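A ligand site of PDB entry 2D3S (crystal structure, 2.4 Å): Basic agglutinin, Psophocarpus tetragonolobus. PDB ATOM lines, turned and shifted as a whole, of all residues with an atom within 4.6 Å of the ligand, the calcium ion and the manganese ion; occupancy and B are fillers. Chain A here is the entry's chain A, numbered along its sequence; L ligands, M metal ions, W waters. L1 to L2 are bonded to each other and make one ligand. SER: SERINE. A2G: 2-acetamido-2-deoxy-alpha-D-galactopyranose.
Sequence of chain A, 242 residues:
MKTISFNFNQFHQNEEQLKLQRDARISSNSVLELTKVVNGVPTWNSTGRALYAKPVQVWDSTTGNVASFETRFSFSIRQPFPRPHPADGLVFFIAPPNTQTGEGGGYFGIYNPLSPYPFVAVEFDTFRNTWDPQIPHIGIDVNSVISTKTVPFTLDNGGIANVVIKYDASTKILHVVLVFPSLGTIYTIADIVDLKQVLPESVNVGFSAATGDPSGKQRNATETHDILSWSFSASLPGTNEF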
ATOM      1  N   HIS A  85     -15.053 -20.141 -25.088  1.00  0.00           N
ATOM      2  CA  HIS A  85     -13.957 -21.055 -25.336  1.00  0.00           C
ATOM      3  C   HIS A  85     -13.344 -21.591 -24.032  1.00  0.00           C
ATOM      4  O   HIS A  85     -12.927 -20.819 -23.173  1.00  0.00           O
ATOM      5  CB  HIS A  85     -12.873 -20.385 -26.200  1.00  0.00           C
ATOM      6  CG  HIS A  85     -12.530 -18.993 -25.776  1.00  0.00           C
ATOM      7  ND1 HIS A  85     -12.487 -17.937 -26.657  1.00  0.00           N
ATOM      8  CD2 HIS A  85     -12.167 -18.483 -24.574  1.00  0.00           C
ATOM      9  CE1 HIS A  85     -12.127 -16.838 -26.022  1.00  0.00           C
ATOM     10  NE2 HIS A  85     -11.920 -17.148 -24.745  1.00  0.00           N
ATOM     11  N   ALA A  87     -10.720 -23.212 -21.375  1.00  0.00           N
ATOM     12  CA  ALA A  87      -9.288 -22.965 -21.194  1.00  0.00           C
ATOM     13  C   ALA A  87      -8.883 -23.416 -19.794  1.00  0.00           C
ATOM     14  O   ALA A  87      -9.733 -23.467 -18.901  1.00  0.00           O
ATOM     15  CB  ALA A  87      -9.014 -21.469 -21.365  1.00  0.00           C
ATOM     16  N   ASP A  88      -7.603 -23.759 -19.585  1.00  0.00           N
ATOM     17  CA  ASP A  88      -6.574 -23.744 -20.626  1.00  0.00           C
ATOM     18  C   ASP A  88      -6.050 -25.142 -20.978  1.00  0.00           C
ATOM     19  O   ASP A  88      -5.659 -25.405 -22.119  1.00  0.00           O
ATOM     20  CB  ASP A  88      -5.387 -22.866 -20.192  1.00  0.00           C
ATOM     21  CG  ASP A  88      -5.570 -21.422 -20.601  1.00  0.00           C
ATOM     22  OD1 ASP A  88      -6.071 -20.617 -19.781  1.00  0.00           O
ATOM     23  OD2 ASP A  88      -5.230 -21.089 -21.757  1.00  0.00           O
ATOM     24  N   GLY A 104      -0.008 -18.560 -15.202  1.00  0.00           N
ATOM     25  CA  GLY A 104      -1.195 -19.358 -15.467  1.00  0.00           C
ATOM     26  C   GLY A 104      -1.556 -19.223 -16.925  1.00  0.00           C
ATOM     27  O   GLY A 104      -0.687 -19.040 -17.772  1.00  0.00           O
ATOM     28  N   GLY A 105      -2.840 -19.319 -17.243  1.00  0.00           N
ATOM     29  CA  GLY A 105      -3.276 -19.203 -18.619  1.00  0.00           C
ATOM     30  C   GLY A 105      -2.597 -20.199 -19.548  1.00  0.00           C
ATOM     31  O   GLY A 105      -2.350 -21.347 -19.171  1.00  0.00           O
ATOM     32  N   GLY A 106      -2.293 -19.747 -20.768  1.00  0.00           N
ATOM     33  CA  GLY A 106      -1.657 -20.605 -21.749  1.00  0.00           C
ATOM     34  C   GLY A 106      -0.314 -21.174 -21.351  1.00  0.00           C
ATOM     35  O   GLY A 106       0.282 -21.942 -22.110  1.00  0.00           O
ATOM     36  N   TYR A 107       0.190 -20.787 -20.184  1.00  0.00           N
ATOM     37  CA  TYR A 107       1.481 -21.304 -19.717  1.00  0.00           C
ATOM     38  C   TYR A 107       1.321 -22.436 -18.690  1.00  0.00           C
ATOM     39  O   TYR A 107       2.303 -22.927 -18.131  1.00  0.00           O
ATOM     40  CB  TYR A 107       2.321 -20.170 -19.134  1.00  0.00           C
ATOM     41  CG  TYR A 107       2.713 -19.158 -20.173  1.00  0.00           C
ATOM     42  CD1 TYR A 107       3.569 -19.509 -21.219  1.00  0.00           C
ATOM     43  CD2 TYR A 107       2.204 -17.862 -20.145  1.00  0.00           C
ATOM     44  CE1 TYR A 107       3.902 -18.596 -22.216  1.00  0.00           C
ATOM     45  CE2 TYR A 107       2.518 -16.936 -21.134  1.00  0.00           C
ATOM     46  CZ  TYR A 107       3.364 -17.308 -22.166  1.00  0.00           C
ATOM     47  OH  TYR A 107       3.673 -16.393 -23.147  1.00  0.00           O
ATOM     48  N   PHE A 108       0.072 -22.828 -18.471  1.00  0.00           N
ATOM     49  CA  PHE A 108      -0.283 -23.922 -17.581  1.00  0.00           C
ATOM     50  C   PHE A 108       0.249 -23.863 -16.155  1.00  0.00           C
ATOM     51  O   PHE A 108      -0.006 -24.763 -15.356  1.00  0.00           O
ATOM     52  CB  PHE A 108       0.175 -25.241 -18.220  1.00  0.00           C
ATOM     53  CG  PHE A 108      -0.254 -25.421 -19.649  1.00  0.00           C
ATOM     54  CD1 PHE A 108      -1.602 -25.521 -19.974  1.00  0.00           C
ATOM     55  CD2 PHE A 108       0.693 -25.550 -20.659  1.00  0.00           C
ATOM     56  CE1 PHE A 108      -1.997 -25.764 -21.299  1.00  0.00           C
ATOM     57  CE2 PHE A 108       0.309 -25.786 -21.981  1.00  0.00           C
ATOM     58  CZ  PHE A 108      -1.043 -25.897 -22.298  1.00  0.00           C
ATOM     59  N   GLU A 123       1.470 -31.921 -22.698  1.00  0.00           N
ATOM     60  CA  GLU A 123       0.277 -31.128 -22.513  1.00  0.00           C
ATOM     61  C   GLU A 123      -0.971 -31.655 -23.222  1.00  0.00           C
ATOM     62  O   GLU A 123      -0.898 -32.335 -24.257  1.00  0.00           O
ATOM     63  CB  GLU A 123       0.524 -29.692 -23.003  1.00  0.00           C
ATOM     64  CG  GLU A 123       0.886 -29.643 -24.479  1.00  0.00           C
ATOM     65  CD  GLU A 123       0.914 -28.241 -25.039  1.00  0.00           C
ATOM     66  OE1 GLU A 123       1.650 -27.375 -24.502  1.00  0.00           O
ATOM     67  OE2 GLU A 123       0.208 -28.021 -26.039  1.00  0.00           O
ATOM     68  N   ASP A 125      -3.777 -29.607 -24.328  1.00  0.00           N
ATOM     69  CA  ASP A 125      -4.166 -28.241 -24.572  1.00  0.00           C
ATOM     70  C   ASP A 125      -5.575 -28.017 -25.103  1.00  0.00           C
ATOM     71  O   ASP A 125      -5.936 -28.527 -26.159  1.00  0.00           O
ATOM     72  CB  ASP A 125      -3.167 -27.642 -25.542  1.00  0.00           C
ATOM     73  CG  ASP A 125      -3.064 -26.156 -25.414  1.00  0.00           C
ATOM     74  OD1 ASP A 125      -4.087 -25.503 -25.125  1.00  0.00           O
ATOM     75  OD2 ASP A 125      -1.946 -25.652 -25.607  1.00  0.00           O
ATOM     76  N   PHE A 127      -7.068 -24.684 -25.274  1.00  0.00           N
ATOM     77  CA  PHE A 127      -7.272 -23.324 -25.754  1.00  0.00           C
ATOM     78  C   PHE A 127      -6.215 -22.928 -26.782  1.00  0.00           C
ATOM     79  O   PHE A 127      -5.030 -23.122 -26.564  1.00  0.00           O
ATOM     80  CB  PHE A 127      -7.234 -22.331 -24.592  1.00  0.00           C
ATOM     81  CG  PHE A 127      -7.413 -20.901 -25.034  1.00  0.00           C
ATOM     82  CD1 PHE A 127      -8.690 -20.386 -25.267  1.00  0.00           C
ATOM     83  CD2 PHE A 127      -6.299 -20.083 -25.263  1.00  0.00           C
ATOM     84  CE1 PHE A 127      -8.856 -19.070 -25.734  1.00  0.00           C
ATOM     85  CE2 PHE A 127      -6.459 -18.779 -25.730  1.00  0.00           C
ATOM     86  CZ  PHE A 127      -7.735 -18.272 -25.975  1.00  0.00           C
ATOM     87  N   ASN A 129      -3.758 -20.657 -28.191  1.00  0.00           N
ATOM     88  CA  ASN A 129      -2.989 -19.436 -27.966  1.00  0.00           C
ATOM     89  C   ASN A 129      -2.391 -19.045 -29.309  1.00  0.00           C
ATOM     90  O   ASN A 129      -2.435 -19.840 -30.255  1.00  0.00           O
ATOM     91  CB  ASN A 129      -1.906 -19.687 -26.928  1.00  0.00           C
ATOM     92  CG  ASN A 129      -2.386 -19.461 -25.513  1.00  0.00           C
ATOM     93  OD1 ASN A 129      -2.327 -18.336 -24.982  1.00  0.00           O
ATOM     94  ND2 ASN A 129      -2.887 -20.514 -24.883  1.00  0.00           N
ATOM     95  N   THR A 130      -1.837 -17.845 -29.413  1.00  0.00           N
ATOM     96  CA  THR A 130      -1.260 -17.401 -30.680  1.00  0.00           C
ATOM     97  C   THR A 130      -0.293 -18.441 -31.261  1.00  0.00           C
ATOM     98  O   THR A 130      -0.222 -18.616 -32.480  1.00  0.00           O
ATOM     99  CB  THR A 130      -0.487 -16.048 -30.538  1.00  0.00           C
ATOM    100  OG1 THR A 130       0.607 -16.202 -29.618  1.00  0.00           O
ATOM    101  CG2 THR A 130      -1.427 -14.951 -30.056  1.00  0.00           C
ATOM    102  N   TRP A 131       0.398 -19.139 -30.370  1.00  0.00           N
ATOM    103  CA  TRP A 131       1.390 -20.142 -30.762  1.00  0.00           C
ATOM    104  C   TRP A 131       0.892 -21.584 -30.920  1.00  0.00           C
ATOM    105  O   TRP A 131       1.721 -22.479 -31.035  1.00  0.00           O
ATOM    106  CB  TRP A 131       2.518 -20.149 -29.737  1.00  0.00           C
ATOM    107  CG  TRP A 131       2.051 -20.596 -28.391  1.00  0.00           C
ATOM    108  CD1 TRP A 131       1.747 -21.868 -28.005  1.00  0.00           C
ATOM    109  CD2 TRP A 131       1.782 -19.761 -27.257  1.00  0.00           C
ATOM    110  NE1 TRP A 131       1.294 -21.885 -26.715  1.00  0.00           N
ATOM    111  CE2 TRP A 131       1.304 -20.602 -26.224  1.00  0.00           C
ATOM    112  CE3 TRP A 131       1.880 -18.384 -27.012  1.00  0.00           C
ATOM    113  CZ2 TRP A 131       0.936 -20.115 -24.971  1.00  0.00           C
ATOM    114  CZ3 TRP A 131       1.522 -17.900 -25.756  1.00  0.00           C
ATOM    115  CH2 TRP A 131       1.051 -18.769 -24.747  1.00  0.00           C
ATOM    116  N   ASP A 132      -0.413 -21.818 -30.922  1.00  0.00           N
ATOM    117  CA  ASP A 132      -0.916 -23.189 -31.060  1.00  0.00           C
ATOM    118  C   ASP A 132      -1.607 -23.502 -32.346  1.00  0.00           C
ATOM    119  O   ASP A 132      -2.087 -22.613 -33.051  1.00  0.00           O
ATOM    120  CB  ASP A 132      -1.958 -23.545 -29.991  1.00  0.00           C
ATOM    121  CG  ASP A 132      -1.439 -23.444 -28.593  1.00  0.00           C
ATOM    122  OD1 ASP A 132      -0.364 -23.984 -28.299  1.00  0.00           O
ATOM    123  OD2 ASP A 132      -2.140 -22.817 -27.788  1.00  0.00           O
ATOM    124  N   HIS A 137      -5.313 -30.540 -28.457  1.00  0.00           N
ATOM    125  CA  HIS A 137      -4.211 -31.318 -28.996  1.00  0.00           C
ATOM    126  C   HIS A 137      -3.272 -31.748 -27.885  1.00  0.00           C
ATOM    127  O   HIS A 137      -3.218 -31.127 -26.828  1.00  0.00           O
ATOM    128  CB  HIS A 137      -3.437 -30.536 -30.057  1.00  0.00           C
ATOM    129  CG  HIS A 137      -2.859 -29.240 -29.567  1.00  0.00           C
ATOM    130  ND1 HIS A 137      -3.428 -28.016 -29.868  1.00  0.00           N
ATOM    131  CD2 HIS A 137      -1.775 -28.968 -28.802  1.00  0.00           C
ATOM    132  CE1 HIS A 137      -2.711 -27.055 -29.310  1.00  0.00           C
ATOM    133  NE2 HIS A 137      -1.704 -27.605 -28.649  1.00  0.00           N
ATOM    134  N   VAL A 145       6.384 -23.818 -24.179  1.00  0.00           N
ATOM    135  CA  VAL A 145       5.007 -24.237 -24.362  1.00  0.00           C
ATOM    136  C   VAL A 145       4.727 -24.324 -25.864  1.00  0.00           C
ATOM    137  O   VAL A 145       3.628 -24.664 -26.299  1.00  0.00           O
ATOM    138  CB  VAL A 145       4.046 -23.244 -23.672  1.00  0.00           C
ATOM    139  CG1 VAL A 145       2.653 -23.343 -24.237  1.00  0.00           C
ATOM    140  CG2 VAL A 145       4.006 -23.549 -22.175  1.00  0.00           C
ATOM    141  N   SER A 147       5.158 -26.426 -28.444  1.00  0.00           N
ATOM    142  CA  SER A 147       5.417 -27.854 -28.638  1.00  0.00           C
ATOM    143  C   SER A 147       6.304 -28.226 -29.816  1.00  0.00           C
ATOM    144  O   SER A 147       6.198 -27.666 -30.904  1.00  0.00           O
ATOM    145  CB  SER A 147       4.091 -28.602 -28.775  1.00  0.00           C
ATOM    146  OG  SER A 147       3.237 -28.291 -27.692  1.00  0.00           O
ATOM    147  N   THR A 211      -6.934 -22.379 -15.712  1.00  0.00           N
ATOM    148  CA  THR A 211      -8.180 -22.021 -16.369  1.00  0.00           C
ATOM    149  C   THR A 211      -7.992 -20.610 -16.919  1.00  0.00           C
ATOM    150  O   THR A 211      -6.948 -19.998 -16.697  1.00  0.00           O
ATOM    151  CB  THR A 211      -9.384 -22.053 -15.385  1.00  0.00           C
ATOM    152  OG1 THR A 211      -9.160 -21.116 -14.330  1.00  0.00           O
ATOM    153  CG2 THR A 211      -9.539 -23.471 -14.796  1.00  0.00           C
ATOM    154  N   GLY A 212      -8.990 -20.103 -17.636  1.00  0.00           N
ATOM    155  CA  GLY A 212      -8.913 -18.778 -18.238  1.00  0.00           C
ATOM    156  C   GLY A 212      -8.287 -17.661 -17.419  1.00  0.00           C
ATOM    157  O   GLY A 212      -8.654 -17.425 -16.276  1.00  0.00           O
ATOM    158  N   ASP A 213      -7.334 -16.970 -18.032  1.00  0.00           N
ATOM    159  CA  ASP A 213      -6.668 -15.853 -17.359  1.00  0.00           C
ATOM    160  C   ASP A 213      -7.544 -14.601 -17.472  1.00  0.00           C
ATOM    161  O   ASP A 213      -8.186 -14.369 -18.507  1.00  0.00           O
ATOM    162  CB  ASP A 213      -5.313 -15.593 -18.019  1.00  0.00           C
ATOM    163  CG  ASP A 213      -4.508 -14.544 -17.290  1.00  0.00           C
ATOM    164  OD1 ASP A 213      -4.048 -14.823 -16.163  1.00  0.00           O
ATOM    165  OD2 ASP A 213      -4.335 -13.441 -17.860  1.00  0.00           O
ATOM    166  N   SER A 215      -6.958 -11.550 -18.120  1.00  0.00           N
ATOM    167  CA  SER A 215      -6.644 -10.752 -19.295  1.00  0.00           C
ATOM    168  C   SER A 215      -7.534 -11.097 -20.490  1.00  0.00           C
ATOM    169  O   SER A 215      -7.686 -10.289 -21.406  1.00  0.00           O
ATOM    170  CB  SER A 215      -5.166 -10.920 -19.687  1.00  0.00           C
ATOM    171  OG  SER A 215      -4.895 -12.241 -20.144  1.00  0.00           O
ATOM    172  N   GLY A 216      -8.109 -12.291 -20.484  1.00  0.00           N
ATOM    173  CA  GLY A 216      -8.967 -12.708 -21.578  1.00  0.00           C
ATOM    174  C   GLY A 216     -10.355 -12.096 -21.492  1.00  0.00           C
ATOM    175  O   GLY A 216     -11.149 -12.195 -22.427  1.00  0.00           O
ATOM    176  N   GLN A 218     -12.926 -13.059 -20.142  1.00  0.00           N
ATOM    177  CA  GLN A 218     -13.991 -14.049 -20.301  1.00  0.00           C
ATOM    178  C   GLN A 218     -14.025 -15.022 -19.134  1.00  0.00           C
ATOM    179  O   GLN A 218     -13.126 -15.848 -18.971  1.00  0.00           O
ATOM    180  CB  GLN A 218     -13.795 -14.827 -21.611  1.00  0.00           C
ATOM    181  CG  GLN A 218     -13.997 -13.987 -22.858  1.00  0.00           C
ATOM    182  CD  GLN A 218     -15.454 -13.662 -23.115  1.00  0.00           C
ATOM    183  OE1 GLN A 218     -16.240 -13.515 -22.186  1.00  0.00           O
ATOM    184  NE2 GLN A 218     -15.815 -13.545 -24.388  1.00  0.00           N
ATOM    185  N   ALA A 221     -14.199 -18.882 -19.862  1.00  0.00           N
ATOM    186  CA  ALA A 221     -12.989 -19.583 -20.299  1.00  0.00           C
ATOM    187  C   ALA A 221     -12.433 -20.449 -19.154  1.00  0.00           C
ATOM    188  O   ALA A 221     -11.375 -20.166 -18.603  1.00  0.00           O
ATOM    189  CB  ALA A 221     -11.954 -18.579 -20.749  1.00  0.00           C
HETATM  190  N   SER L   1      -7.014 -14.126 -26.192  1.00  0.00           N
HETATM  191  CA  SER L   1      -5.805 -13.529 -25.607  1.00  0.00           C
HETATM  192  C   SER L   1      -4.526 -14.207 -26.138  1.00  0.00           C
HETATM  193  O   SER L   1      -3.408 -13.880 -25.711  1.00  0.00           O
HETATM  194  CB  SER L   1      -5.897 -13.629 -24.071  1.00  0.00           C
HETATM  195  OG  SER L   1      -5.806 -14.979 -23.649  1.00  0.00           O
HETATM  196  OXT SER L   1      -4.592 -15.097 -27.010  1.00  0.00           O
HETATM  197  O5  A2G L   2      -6.989 -15.610 -21.730  1.00  0.00           O
HETATM  198  C1  A2G L   2      -5.682 -15.272 -22.255  1.00  0.00           C
HETATM  199  C2  A2G L   2      -4.709 -16.445 -22.084  1.00  0.00           C
HETATM  200  N2  A2G L   2      -3.431 -16.059 -22.651  1.00  0.00           N
HETATM  201  C3  A2G L   2      -5.284 -17.698 -22.775  1.00  0.00           C
HETATM  202  O3  A2G L   2      -4.390 -18.794 -22.623  1.00  0.00           O
HETATM  203  C4  A2G L   2      -6.642 -18.033 -22.158  1.00  0.00           C
HETATM  204  O4  A2G L   2      -6.450 -18.319 -20.777  1.00  0.00           O
HETATM  205  C5  A2G L   2      -7.558 -16.811 -22.329  1.00  0.00           C
HETATM  206  C6  A2G L   2      -8.924 -17.069 -21.713  1.00  0.00           C
HETATM  207  O6  A2G L   2      -9.798 -16.007 -22.116  1.00  0.00           O
HETATM  208  C7  A2G L   2      -2.285 -16.093 -21.959  1.00  0.00           C
HETATM  209  O7  A2G L   2      -2.246 -16.472 -20.798  1.00  0.00           O
HETATM  210  C8  A2G L   2      -1.061 -15.653 -22.709  1.00  0.00           C
HETATM  211 CA    CA M   1      -2.827 -23.147 -25.364  1.00  0.00          CA
HETATM  212 MN    MN M   2      -0.446 -26.128 -27.323  1.00  0.00          MN
HETATM  213  O   HOH W   1      -0.473 -23.331 -24.244  1.00  0.00           O
HETATM  214  O   HOH W   2       1.459 -26.534 -28.478  1.00  0.00           O
HETATM  215  O   HOH W   3      -3.661 -23.100 -22.752  1.00  0.00           O
HETATM  216  O   HOH W   4      -1.967 -16.191 -26.680  1.00  0.00           O
HETATM  217  O   HOH W   5     -10.579 -14.988 -19.530  1.00  0.00           O
HETATM  218  O   HOH W   6      -6.953 -11.444 -27.821  1.00  0.00           O
HETATM  219  O   HOH W   7       0.914 -25.080 -25.985  1.00  0.00           O
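His 85 touches the ligand. Gly 105 touches the ligand. Gly 212 touches the ligand. OG of Ser 215 touches C1 of A2G L2, 3.8 Å away. Gly 216 touches the ligand. CB of Ala 221 touches C6 of A2G L2 (3.5 Å). Hydrophobic or aromatic side chains that line the ligand: Phe 127 and Ala 221. 11 residues have an atom within 4 Å of the ligand: His 85, Asp 88, Gly 105, Gly 106, Phe 127, Asn 129, Gly 212, Asp 213, Ser 215, Gly 216 and Ala 221.
The side-chain hydroxyl of Ser 215 lies within hydrogen-bond range of the side-chain carboxylate of Asp 213, 2.6 Å away. The backbone NH (N) of Gly 106 lies within hydrogen-bond range of the side-chain carboxylate (OD2) of Asp 88 (3.4 Å). The side-chain hydroxyl of Ser 147 sits close to the side-chain carboxylate of Glu 123 (3.5 Å). The side-chain carboxylate of Asp 132 sits close to the indole nitrogen of Trp 131 (3.1 Å). The backbone carbonyl oxygen (O) of Ala 221 lies within hydrogen-bond range of the backbone NH (N) of Gly 212.
OD1 of Asn 129 lies within hydrogen-bond range of O3 of A2G L2 (3.2 Å). OD1 of Asp 88 lies within hydrogen-bond range of O4 of A2G L2. The backbone NH (N) of Asp 213 is in hydrogen-bond range of an oxygen (O4) of A2G L2 (3.2 Å). O3 of A2G L2 is in hydrogen-bond range of N of Gly 106 (3.0 Å).
Water W1 lies within hydrogen-bond range of the backbone carbonyl oxygen of Gly 106 and the indole nitrogen of Trp 131. Water W7 lies within hydrogen-bond range of O of Val 145, OE1 of Glu 123 and NE1 of Trp 131. Water W4 lies within hydrogen-bond range of OD1 of Asn 129, OXT of SER L1 and N of Thr 130. Water W5 lies within hydrogen-bond range of O of Asp 213, O of Gln 218 and O6 of A2G L2.
The manganese ion is bound by water W7, water W2, OD2 of Asp 125, NE2 of His 137, OD1 of Asp 132 and OE2 of Glu 123.
Within 4 Å of the calcium ion: Asp 125, Phe 127, Asn 129 and Asp 132. Along chain A the residues within 4 Å of the calcium ion span positions 125 to 132. The nearest printed residue that does not touch the calcium ion is Phe 108 (4.5 Å).
Within 4 Å of the manganese ion: Glu 123, Asp 125, Asp 132 and His 137. Along chain A the residues within 4 Å of the manganese ion span positions 123 to 137. The nearest printed residue that does not touch the manganese ion is Ser 147 (4.3 Å).
The calcium ion is bound by the backbone carbonyl oxygen (O) of Phe 127 (2.5 Å), the side-chain carboxylate (OD2) of Asp 132 (2.5 Å), water W1 (2.6 Å), the side-chain carboxylate (OD2) of Asp 125 (2.7 Å), the side-chain amide nitrogen (ND2) of Asn 129 (2.7 Å), the side-chain carboxylate (OD1) of Asp 125 (2.7 Å) and water W3 (2.7 Å). The calcium ion has seven donor atoms within binding distance.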
